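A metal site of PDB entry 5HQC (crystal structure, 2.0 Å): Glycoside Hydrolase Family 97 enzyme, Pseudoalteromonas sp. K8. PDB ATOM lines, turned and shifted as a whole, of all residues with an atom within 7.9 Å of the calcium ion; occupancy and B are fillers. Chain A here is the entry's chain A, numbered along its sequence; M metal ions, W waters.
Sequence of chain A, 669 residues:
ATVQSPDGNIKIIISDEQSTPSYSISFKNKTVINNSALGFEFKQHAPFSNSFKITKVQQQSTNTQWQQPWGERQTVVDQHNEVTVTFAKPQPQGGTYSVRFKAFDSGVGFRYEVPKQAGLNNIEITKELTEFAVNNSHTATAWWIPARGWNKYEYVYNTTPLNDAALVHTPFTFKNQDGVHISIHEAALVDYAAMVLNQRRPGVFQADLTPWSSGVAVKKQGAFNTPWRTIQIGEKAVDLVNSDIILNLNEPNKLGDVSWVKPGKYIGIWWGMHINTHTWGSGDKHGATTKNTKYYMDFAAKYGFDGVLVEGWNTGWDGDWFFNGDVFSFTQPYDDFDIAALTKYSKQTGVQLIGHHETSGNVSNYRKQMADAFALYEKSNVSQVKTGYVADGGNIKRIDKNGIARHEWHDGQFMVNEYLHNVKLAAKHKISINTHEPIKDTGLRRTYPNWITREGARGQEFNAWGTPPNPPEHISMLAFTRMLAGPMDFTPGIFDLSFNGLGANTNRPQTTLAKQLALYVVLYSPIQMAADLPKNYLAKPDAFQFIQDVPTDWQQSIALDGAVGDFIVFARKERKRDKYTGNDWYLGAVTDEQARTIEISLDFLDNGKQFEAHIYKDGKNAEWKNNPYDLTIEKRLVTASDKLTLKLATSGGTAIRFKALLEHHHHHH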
ATOM      1  N   LYS A 152      -3.690  19.955 -17.174  1.00  0.00           N
ATOM      2  CA  LYS A 152      -4.129  18.708 -16.520  1.00  0.00           C
ATOM      3  C   LYS A 152      -5.403  18.198 -17.198  1.00  0.00           C
ATOM      4  O   LYS A 152      -5.374  18.003 -18.425  1.00  0.00           O
ATOM      5  CB  LYS A 152      -4.230  18.957 -15.014  1.00  0.00           C
ATOM      6  CG  LYS A 152      -2.977  19.653 -14.455  1.00  0.00           C
ATOM      7  CD  LYS A 152      -3.007  19.784 -12.948  1.00  0.00           C
ATOM      8  CE  LYS A 152      -4.091  20.728 -12.426  1.00  0.00           C
ATOM      9  NZ  LYS A 152      -3.952  22.129 -12.894  1.00  0.00           N
ATOM     10  N   GLU A 154      -8.217  19.924 -17.320  1.00  0.00           N
ATOM     11  CA  GLU A 154      -9.093  21.079 -17.570  1.00  0.00           C
ATOM     12  C   GLU A 154      -8.868  21.644 -18.969  1.00  0.00           C
ATOM     13  O   GLU A 154      -8.312  22.732 -19.155  1.00  0.00           O
ATOM     14  CB  GLU A 154      -8.862  22.147 -16.502  1.00  0.00           C
ATOM     15  CG  GLU A 154      -9.435  21.798 -15.142  1.00  0.00           C
ATOM     16  CD  GLU A 154      -8.674  20.681 -14.485  1.00  0.00           C
ATOM     17  OE1 GLU A 154      -9.305  19.736 -13.953  1.00  0.00           O
ATOM     18  OE2 GLU A 154      -7.422  20.724 -14.477  1.00  0.00           O
ATOM     19  N   TRP A 270     -17.836  31.884  -2.876  1.00  0.00           N
ATOM     20  CA  TRP A 270     -17.077  31.187  -3.896  1.00  0.00           C
ATOM     21  C   TRP A 270     -17.102  31.927  -5.225  1.00  0.00           C
ATOM     22  O   TRP A 270     -16.077  32.453  -5.661  1.00  0.00           O
ATOM     23  CB  TRP A 270     -17.625  29.761  -4.085  1.00  0.00           C
ATOM     24  CG  TRP A 270     -16.885  29.027  -5.183  1.00  0.00           C
ATOM     25  CD1 TRP A 270     -15.620  28.516  -5.105  1.00  0.00           C
ATOM     26  CD2 TRP A 270     -17.350  28.761  -6.505  1.00  0.00           C
ATOM     27  NE1 TRP A 270     -15.262  27.946  -6.313  1.00  0.00           N
ATOM     28  CE2 TRP A 270     -16.307  28.087  -7.194  1.00  0.00           C
ATOM     29  CE3 TRP A 270     -18.535  29.028  -7.195  1.00  0.00           C
ATOM     30  CZ2 TRP A 270     -16.426  27.674  -8.524  1.00  0.00           C
ATOM     31  CZ3 TRP A 270     -18.653  28.615  -8.524  1.00  0.00           C
ATOM     32  CH2 TRP A 270     -17.598  27.953  -9.173  1.00  0.00           C
ATOM     33  N   HIS A 274     -14.498  34.420  -7.913  1.00  0.00           N
ATOM     34  CA  HIS A 274     -14.180  34.108  -9.310  1.00  0.00           C
ATOM     35  C   HIS A 274     -14.580  35.242 -10.250  1.00  0.00           C
ATOM     36  O   HIS A 274     -13.925  35.428 -11.286  1.00  0.00           O
ATOM     37  CB  HIS A 274     -14.850  32.797  -9.703  1.00  0.00           C
ATOM     38  CG  HIS A 274     -14.119  31.588  -9.217  1.00  0.00           C
ATOM     39  ND1 HIS A 274     -13.038  31.057  -9.884  1.00  0.00           N
ATOM     40  CD2 HIS A 274     -14.270  30.832  -8.093  1.00  0.00           C
ATOM     41  CE1 HIS A 274     -12.578  30.004  -9.221  1.00  0.00           C
ATOM     42  NE2 HIS A 274     -13.313  29.850  -8.127  1.00  0.00           N
ATOM     43  N   TRP A 321      -2.321  33.825  -4.384  1.00  0.00           N
ATOM     44  CA  TRP A 321      -2.440  32.568  -3.650  1.00  0.00           C
ATOM     45  C   TRP A 321      -1.984  31.370  -4.459  1.00  0.00           C
ATOM     46  O   TRP A 321      -1.650  30.339  -3.863  1.00  0.00           O
ATOM     47  CB  TRP A 321      -3.877  32.370  -3.175  1.00  0.00           C
ATOM     48  CG  TRP A 321      -4.916  32.288  -4.263  1.00  0.00           C
ATOM     49  CD1 TRP A 321      -5.686  33.313  -4.736  1.00  0.00           C
ATOM     50  CD2 TRP A 321      -5.293  31.131  -5.001  1.00  0.00           C
ATOM     51  NE1 TRP A 321      -6.534  32.856  -5.714  1.00  0.00           N
ATOM     52  CE2 TRP A 321      -6.313  31.511  -5.894  1.00  0.00           C
ATOM     53  CE3 TRP A 321      -4.877  29.784  -4.988  1.00  0.00           C
ATOM     54  CZ2 TRP A 321      -6.913  30.615  -6.778  1.00  0.00           C
ATOM     55  CZ3 TRP A 321      -5.478  28.891  -5.855  1.00  0.00           C
ATOM     56  CH2 TRP A 321      -6.487  29.309  -6.736  1.00  0.00           C
ATOM     57  N   GLU A 358      -7.338  24.233   0.281  1.00  0.00           N
ATOM     58  CA  GLU A 358      -6.547  24.451  -0.924  1.00  0.00           C
ATOM     59  C   GLU A 358      -5.065  24.334  -0.572  1.00  0.00           C
ATOM     60  O   GLU A 358      -4.606  24.969   0.382  1.00  0.00           O
ATOM     61  CB  GLU A 358      -6.841  25.827  -1.540  1.00  0.00           C
ATOM     62  CG  GLU A 358      -5.959  26.189  -2.754  1.00  0.00           C
ATOM     63  CD  GLU A 358      -6.074  25.176  -3.903  1.00  0.00           C
ATOM     64  OE1 GLU A 358      -5.061  24.536  -4.260  1.00  0.00           O
ATOM     65  OE2 GLU A 358      -7.179  25.048  -4.473  1.00  0.00           O
ATOM     66  N   LYS A 386     -14.068  20.354   0.750  1.00  0.00           N
ATOM     67  CA  LYS A 386     -13.571  20.508  -0.616  1.00  0.00           C
ATOM     68  C   LYS A 386     -12.060  20.705  -0.550  1.00  0.00           C
ATOM     69  O   LYS A 386     -11.594  21.625   0.132  1.00  0.00           O
ATOM     70  CB  LYS A 386     -14.248  21.704  -1.283  1.00  0.00           C
ATOM     71  CG  LYS A 386     -13.714  22.082  -2.651  1.00  0.00           C
ATOM     72  CD  LYS A 386     -14.458  23.315  -3.184  1.00  0.00           C
ATOM     73  CE  LYS A 386     -14.015  23.681  -4.581  1.00  0.00           C
ATOM     74  NZ  LYS A 386     -14.600  24.977  -5.039  1.00  0.00           N
ATOM     75  N   THR A 387     -11.301  19.850  -1.218  1.00  0.00           N
ATOM     76  CA  THR A 387      -9.849  20.001  -1.273  1.00  0.00           C
ATOM     77  C   THR A 387      -9.444  20.544  -2.636  1.00  0.00           C
ATOM     78  O   THR A 387     -10.224  20.568  -3.595  1.00  0.00           O
ATOM     79  CB  THR A 387      -9.134  18.677  -0.999  1.00  0.00           C
ATOM     80  OG1 THR A 387      -9.519  17.702  -1.983  1.00  0.00           O
ATOM     81  CG2 THR A 387      -9.471  18.182   0.391  1.00  0.00           C
ATOM     82  N   GLY A 388      -8.199  21.008  -2.722  1.00  0.00           N
ATOM     83  CA  GLY A 388      -7.693  21.613  -3.934  1.00  0.00           C
ATOM     84  C   GLY A 388      -6.189  21.489  -4.078  1.00  0.00           C
ATOM     85  O   GLY A 388      -5.451  21.555  -3.089  1.00  0.00           O
ATOM     86  N   TYR A 389      -5.721  21.308  -5.312  1.00  0.00           N
ATOM     87  CA  TYR A 389      -4.319  21.054  -5.603  1.00  0.00           C
ATOM     88  C   TYR A 389      -3.890  21.899  -6.811  1.00  0.00           C
ATOM     89  O   TYR A 389      -3.367  21.390  -7.809  1.00  0.00           O
ATOM     90  CB  TYR A 389      -4.081  19.563  -5.852  1.00  0.00           C
ATOM     91  CG  TYR A 389      -4.474  18.696  -4.673  1.00  0.00           C
ATOM     92  CD1 TYR A 389      -5.806  18.330  -4.457  1.00  0.00           C
ATOM     93  CD2 TYR A 389      -3.523  18.245  -3.763  1.00  0.00           C
ATOM     94  CE1 TYR A 389      -6.180  17.539  -3.364  1.00  0.00           C
ATOM     95  CE2 TYR A 389      -3.885  17.446  -2.656  1.00  0.00           C
ATOM     96  CZ  TYR A 389      -5.218  17.105  -2.468  1.00  0.00           C
ATOM     97  OH  TYR A 389      -5.596  16.316  -1.399  1.00  0.00           O
ATOM     98  N   VAL A 390      -4.088  23.210  -6.701  1.00  0.00           N
ATOM     99  CA  VAL A 390      -3.873  24.123  -7.832  1.00  0.00           C
ATOM    100  C   VAL A 390      -2.379  24.257  -8.104  1.00  0.00           C
ATOM    101  O   VAL A 390      -1.628  24.786  -7.274  1.00  0.00           O
ATOM    102  CB  VAL A 390      -4.518  25.485  -7.555  1.00  0.00           C
ATOM    103  CG1 VAL A 390      -4.073  26.520  -8.610  1.00  0.00           C
ATOM    104  CG2 VAL A 390      -6.041  25.369  -7.534  1.00  0.00           C
ATOM    105  N   THR A 435     -12.883  16.523  -4.242  1.00  0.00           N
ATOM    106  CA  THR A 435     -11.498  16.822  -4.642  1.00  0.00           C
ATOM    107  C   THR A 435     -11.485  17.674  -5.909  1.00  0.00           C
ATOM    108  O   THR A 435     -11.862  17.191  -6.974  1.00  0.00           O
ATOM    109  CB  THR A 435     -10.703  15.546  -4.867  1.00  0.00           C
ATOM    110  OG1 THR A 435     -10.854  14.662  -3.759  1.00  0.00           O
ATOM    111  CG2 THR A 435      -9.209  15.860  -5.050  1.00  0.00           C
ATOM    112  N   HIS A 436     -11.016  18.919  -5.816  1.00  0.00           N
ATOM    113  CA  HIS A 436     -10.699  19.672  -7.025  1.00  0.00           C
ATOM    114  C   HIS A 436      -9.217  19.503  -7.363  1.00  0.00           C
ATOM    115  O   HIS A 436      -8.387  19.262  -6.472  1.00  0.00           O
ATOM    116  CB  HIS A 436     -11.095  21.152  -6.863  1.00  0.00           C
ATOM    117  CG  HIS A 436     -12.578  21.359  -7.018  1.00  0.00           C
ATOM    118  ND1 HIS A 436     -13.120  22.377  -7.776  1.00  0.00           N
ATOM    119  CD2 HIS A 436     -13.632  20.633  -6.559  1.00  0.00           C
ATOM    120  CE1 HIS A 436     -14.431  22.294  -7.742  1.00  0.00           C
ATOM    121  NE2 HIS A 436     -14.774  21.239  -7.016  1.00  0.00           N
ATOM    122  N   GLU A 437      -8.910  19.625  -8.658  1.00  0.00           N
ATOM    123  CA  GLU A 437      -7.626  19.206  -9.202  1.00  0.00           C
ATOM    124  C   GLU A 437      -7.285  17.787  -8.751  1.00  0.00           C
ATOM    125  O   GLU A 437      -6.281  17.562  -8.070  1.00  0.00           O
ATOM    126  CB  GLU A 437      -6.502  20.184  -8.844  1.00  0.00           C
ATOM    127  CG  GLU A 437      -6.935  21.632  -8.569  1.00  0.00           C
ATOM    128  CD  GLU A 437      -7.845  22.218  -9.637  1.00  0.00           C
ATOM    129  OE1 GLU A 437      -8.888  22.810  -9.269  1.00  0.00           O
ATOM    130  OE2 GLU A 437      -7.528  22.104 -10.847  1.00  0.00           O
ATOM    131  N   PRO A 438      -8.109  16.798  -9.112  1.00  0.00           N
ATOM    132  CA  PRO A 438      -7.985  15.461  -8.544  1.00  0.00           C
ATOM    133  C   PRO A 438      -7.231  14.498  -9.442  1.00  0.00           C
ATOM    134  O   PRO A 438      -6.804  14.868 -10.536  1.00  0.00           O
ATOM    135  CB  PRO A 438      -9.443  15.029  -8.446  1.00  0.00           C
ATOM    136  CG  PRO A 438      -9.975  15.525  -9.814  1.00  0.00           C
ATOM    137  CD  PRO A 438      -9.275  16.887 -10.007  1.00  0.00           C
ATOM    138  N   GLU A 455     -13.713  17.352  -9.267  1.00  0.00           N
ATOM    139  CA  GLU A 455     -13.783  18.167 -10.471  1.00  0.00           C
ATOM    140  C   GLU A 455     -13.086  17.434 -11.631  1.00  0.00           C
ATOM    141  O   GLU A 455     -13.714  16.582 -12.267  1.00  0.00           O
ATOM    142  CB  GLU A 455     -13.182  19.556 -10.219  1.00  0.00           C
ATOM    143  CG  GLU A 455     -13.461  20.543 -11.331  1.00  0.00           C
ATOM    144  CD  GLU A 455     -12.944  21.919 -10.973  1.00  0.00           C
ATOM    145  OE1 GLU A 455     -11.728  22.031 -10.808  1.00  0.00           O
ATOM    146  OE2 GLU A 455     -13.757  22.844 -10.807  1.00  0.00           O
ATOM    147  N   GLY A 456     -11.825  17.751 -11.916  1.00  0.00           N
ATOM    148  CA  GLY A 456     -11.123  16.955 -12.931  1.00  0.00           C
ATOM    149  C   GLY A 456     -11.637  17.116 -14.352  1.00  0.00           C
ATOM    150  O   GLY A 456     -11.688  16.133 -15.107  1.00  0.00           O
ATOM    151  N   ALA A 457     -11.996  18.340 -14.728  1.00  0.00           N
ATOM    152  CA  ALA A 457     -12.541  18.744 -16.025  1.00  0.00           C
ATOM    153  C   ALA A 457     -12.836  20.227 -15.861  1.00  0.00           C
ATOM    154  O   ALA A 457     -12.824  20.758 -14.746  1.00  0.00           O
ATOM    155  CB  ALA A 457     -13.820  17.984 -16.412  1.00  0.00           C
ATOM    156  N   ARG A 458     -13.090  20.913 -16.984  1.00  0.00           N
ATOM    157  CA  ARG A 458     -13.475  22.306 -16.896  1.00  0.00           C
ATOM    158  C   ARG A 458     -14.918  22.395 -16.408  1.00  0.00           C
ATOM    159  O   ARG A 458     -15.841  21.900 -17.058  1.00  0.00           O
ATOM    160  CB  ARG A 458     -13.315  23.008 -18.245  1.00  0.00           C
ATOM    161  CG  ARG A 458     -11.847  23.308 -18.615  1.00  0.00           C
ATOM    162  CD  ARG A 458     -11.726  23.881 -20.036  1.00  0.00           C
ATOM    163  NE  ARG A 458     -12.550  25.088 -20.242  1.00  0.00           N
ATOM    164  CZ  ARG A 458     -12.104  26.235 -20.745  1.00  0.00           C
ATOM    165  NH1 ARG A 458     -10.820  26.368 -21.070  1.00  0.00           N
ATOM    166  NH2 ARG A 458     -12.941  27.257 -20.919  1.00  0.00           N
ATOM    167  N   GLY A 459     -15.113  23.021 -15.248  1.00  0.00           N
ATOM    168  CA  GLY A 459     -16.424  23.279 -14.716  1.00  0.00           C
ATOM    169  C   GLY A 459     -16.824  24.733 -14.897  1.00  0.00           C
ATOM    170  O   GLY A 459     -16.250  25.472 -15.702  1.00  0.00           O
ATOM    171  N   GLU A 461     -16.289  27.326 -13.159  1.00  0.00           N
ATOM    172  CA  GLU A 461     -15.306  28.373 -12.870  1.00  0.00           C
ATOM    173  C   GLU A 461     -14.652  28.918 -14.142  1.00  0.00           C
ATOM    174  O   GLU A 461     -14.312  30.108 -14.186  1.00  0.00           O
ATOM    175  CB  GLU A 461     -14.220  27.827 -11.928  1.00  0.00           C
ATOM    176  CG  GLU A 461     -13.472  26.627 -12.514  1.00  0.00           C
ATOM    177  CD  GLU A 461     -12.291  26.187 -11.663  1.00  0.00           C
ATOM    178  OE1 GLU A 461     -11.776  27.007 -10.880  1.00  0.00           O
ATOM    179  OE2 GLU A 461     -11.878  25.020 -11.801  1.00  0.00           O
ATOM    180  N   PHE A 462     -14.476  28.092 -15.173  1.00  0.00           N
ATOM    181  CA  PHE A 462     -13.883  28.580 -16.412  1.00  0.00           C
ATOM    182  C   PHE A 462     -14.791  29.534 -17.167  1.00  0.00           C
ATOM    183  O   PHE A 462     -14.335  30.222 -18.073  1.00  0.00           O
ATOM    184  CB  PHE A 462     -13.492  27.397 -17.329  1.00  0.00           C
ATOM    185  CG  PHE A 462     -12.152  26.797 -16.979  1.00  0.00           C
ATOM    186  CD1 PHE A 462     -12.043  25.865 -15.948  1.00  0.00           C
ATOM    187  CD2 PHE A 462     -11.007  27.170 -17.663  1.00  0.00           C
ATOM    188  CE1 PHE A 462     -10.810  25.321 -15.604  1.00  0.00           C
ATOM    189  CE2 PHE A 462      -9.763  26.635 -17.337  1.00  0.00           C
ATOM    190  CZ  PHE A 462      -9.676  25.711 -16.297  1.00  0.00           C
ATOM    191  N   TRP A 465     -13.671  33.300 -16.136  1.00  0.00           N
ATOM    192  CA  TRP A 465     -12.435  33.937 -16.601  1.00  0.00           C
ATOM    193  C   TRP A 465     -11.700  33.138 -17.660  1.00  0.00           C
ATOM    194  O   TRP A 465     -10.552  33.486 -17.988  1.00  0.00           O
ATOM    195  CB  TRP A 465     -11.482  34.168 -15.397  1.00  0.00           C
ATOM    196  CG  TRP A 465     -11.559  33.045 -14.405  1.00  0.00           C
ATOM    197  CD1 TRP A 465     -12.177  33.063 -13.181  1.00  0.00           C
ATOM    198  CD2 TRP A 465     -11.044  31.714 -14.567  1.00  0.00           C
ATOM    199  NE1 TRP A 465     -12.065  31.829 -12.571  1.00  0.00           N
ATOM    200  CE2 TRP A 465     -11.382  30.983 -13.399  1.00  0.00           C
ATOM    201  CE3 TRP A 465     -10.321  31.073 -15.581  1.00  0.00           C
ATOM    202  CZ2 TRP A 465     -11.025  29.644 -13.216  1.00  0.00           C
ATOM    203  CZ3 TRP A 465      -9.965  29.725 -15.403  1.00  0.00           C
ATOM    204  CH2 TRP A 465     -10.312  29.038 -14.230  1.00  0.00           C
ATOM    205  N   ASP A 489     -18.425  17.582  -9.650  1.00  0.00           N
ATOM    206  CA  ASP A 489     -18.813  18.838  -9.008  1.00  0.00           C
ATOM    207  C   ASP A 489     -18.619  19.947 -10.036  1.00  0.00           C
ATOM    208  O   ASP A 489     -17.587  20.620 -10.078  1.00  0.00           O
ATOM    209  CB  ASP A 489     -17.959  19.062  -7.753  1.00  0.00           C
ATOM    210  CG  ASP A 489     -18.392  20.278  -6.939  1.00  0.00           C
ATOM    211  OD1 ASP A 489     -17.507  21.015  -6.446  1.00  0.00           O
ATOM    212  OD2 ASP A 489     -19.614  20.498  -6.763  1.00  0.00           O
HETATM  213 CA    CA M   1     -10.432  23.872 -10.597  1.00  0.00          CA
HETATM  214  O   HOH W   1      -9.275  23.245 -12.474  1.00  0.00           O
HETATM  215  O   HOH W   2     -11.495  24.313  -8.549  1.00  0.00           O
HETATM  216  O   HOH W   3      -9.309  26.000 -10.087  1.00  0.00           O
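O of Glu 461 lies close to NE1 of Trp 465 (3.3 Å).
A ring nitrogen (ND1) of His 436 sits at hydrogen-bond distance from the side-chain carboxylate (OE2) of Glu 455 (3.1 Å).
The backbone NH (N) of Glu 455 is in hydrogen-bond range of the backbone carbonyl oxygen (O) of Thr 435 (3.0 Å).
The calcium ion is bound by OE2 of Glu 461 (2.2 Å), OE1 of Glu 455 (2.3 Å), water W1 (2.3 Å), OE1 of Glu 437 (2.3 Å), water W2 (2.3 Å) and water W3 (2.5 Å).
The calcium ion has six donor atoms within binding distance.
Within 4 Å of the calcium ion: Glu 437, Glu 455 and Glu 461.
The nearest printed residue that does not touch the calcium ion is His 436 (4.2 Å).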
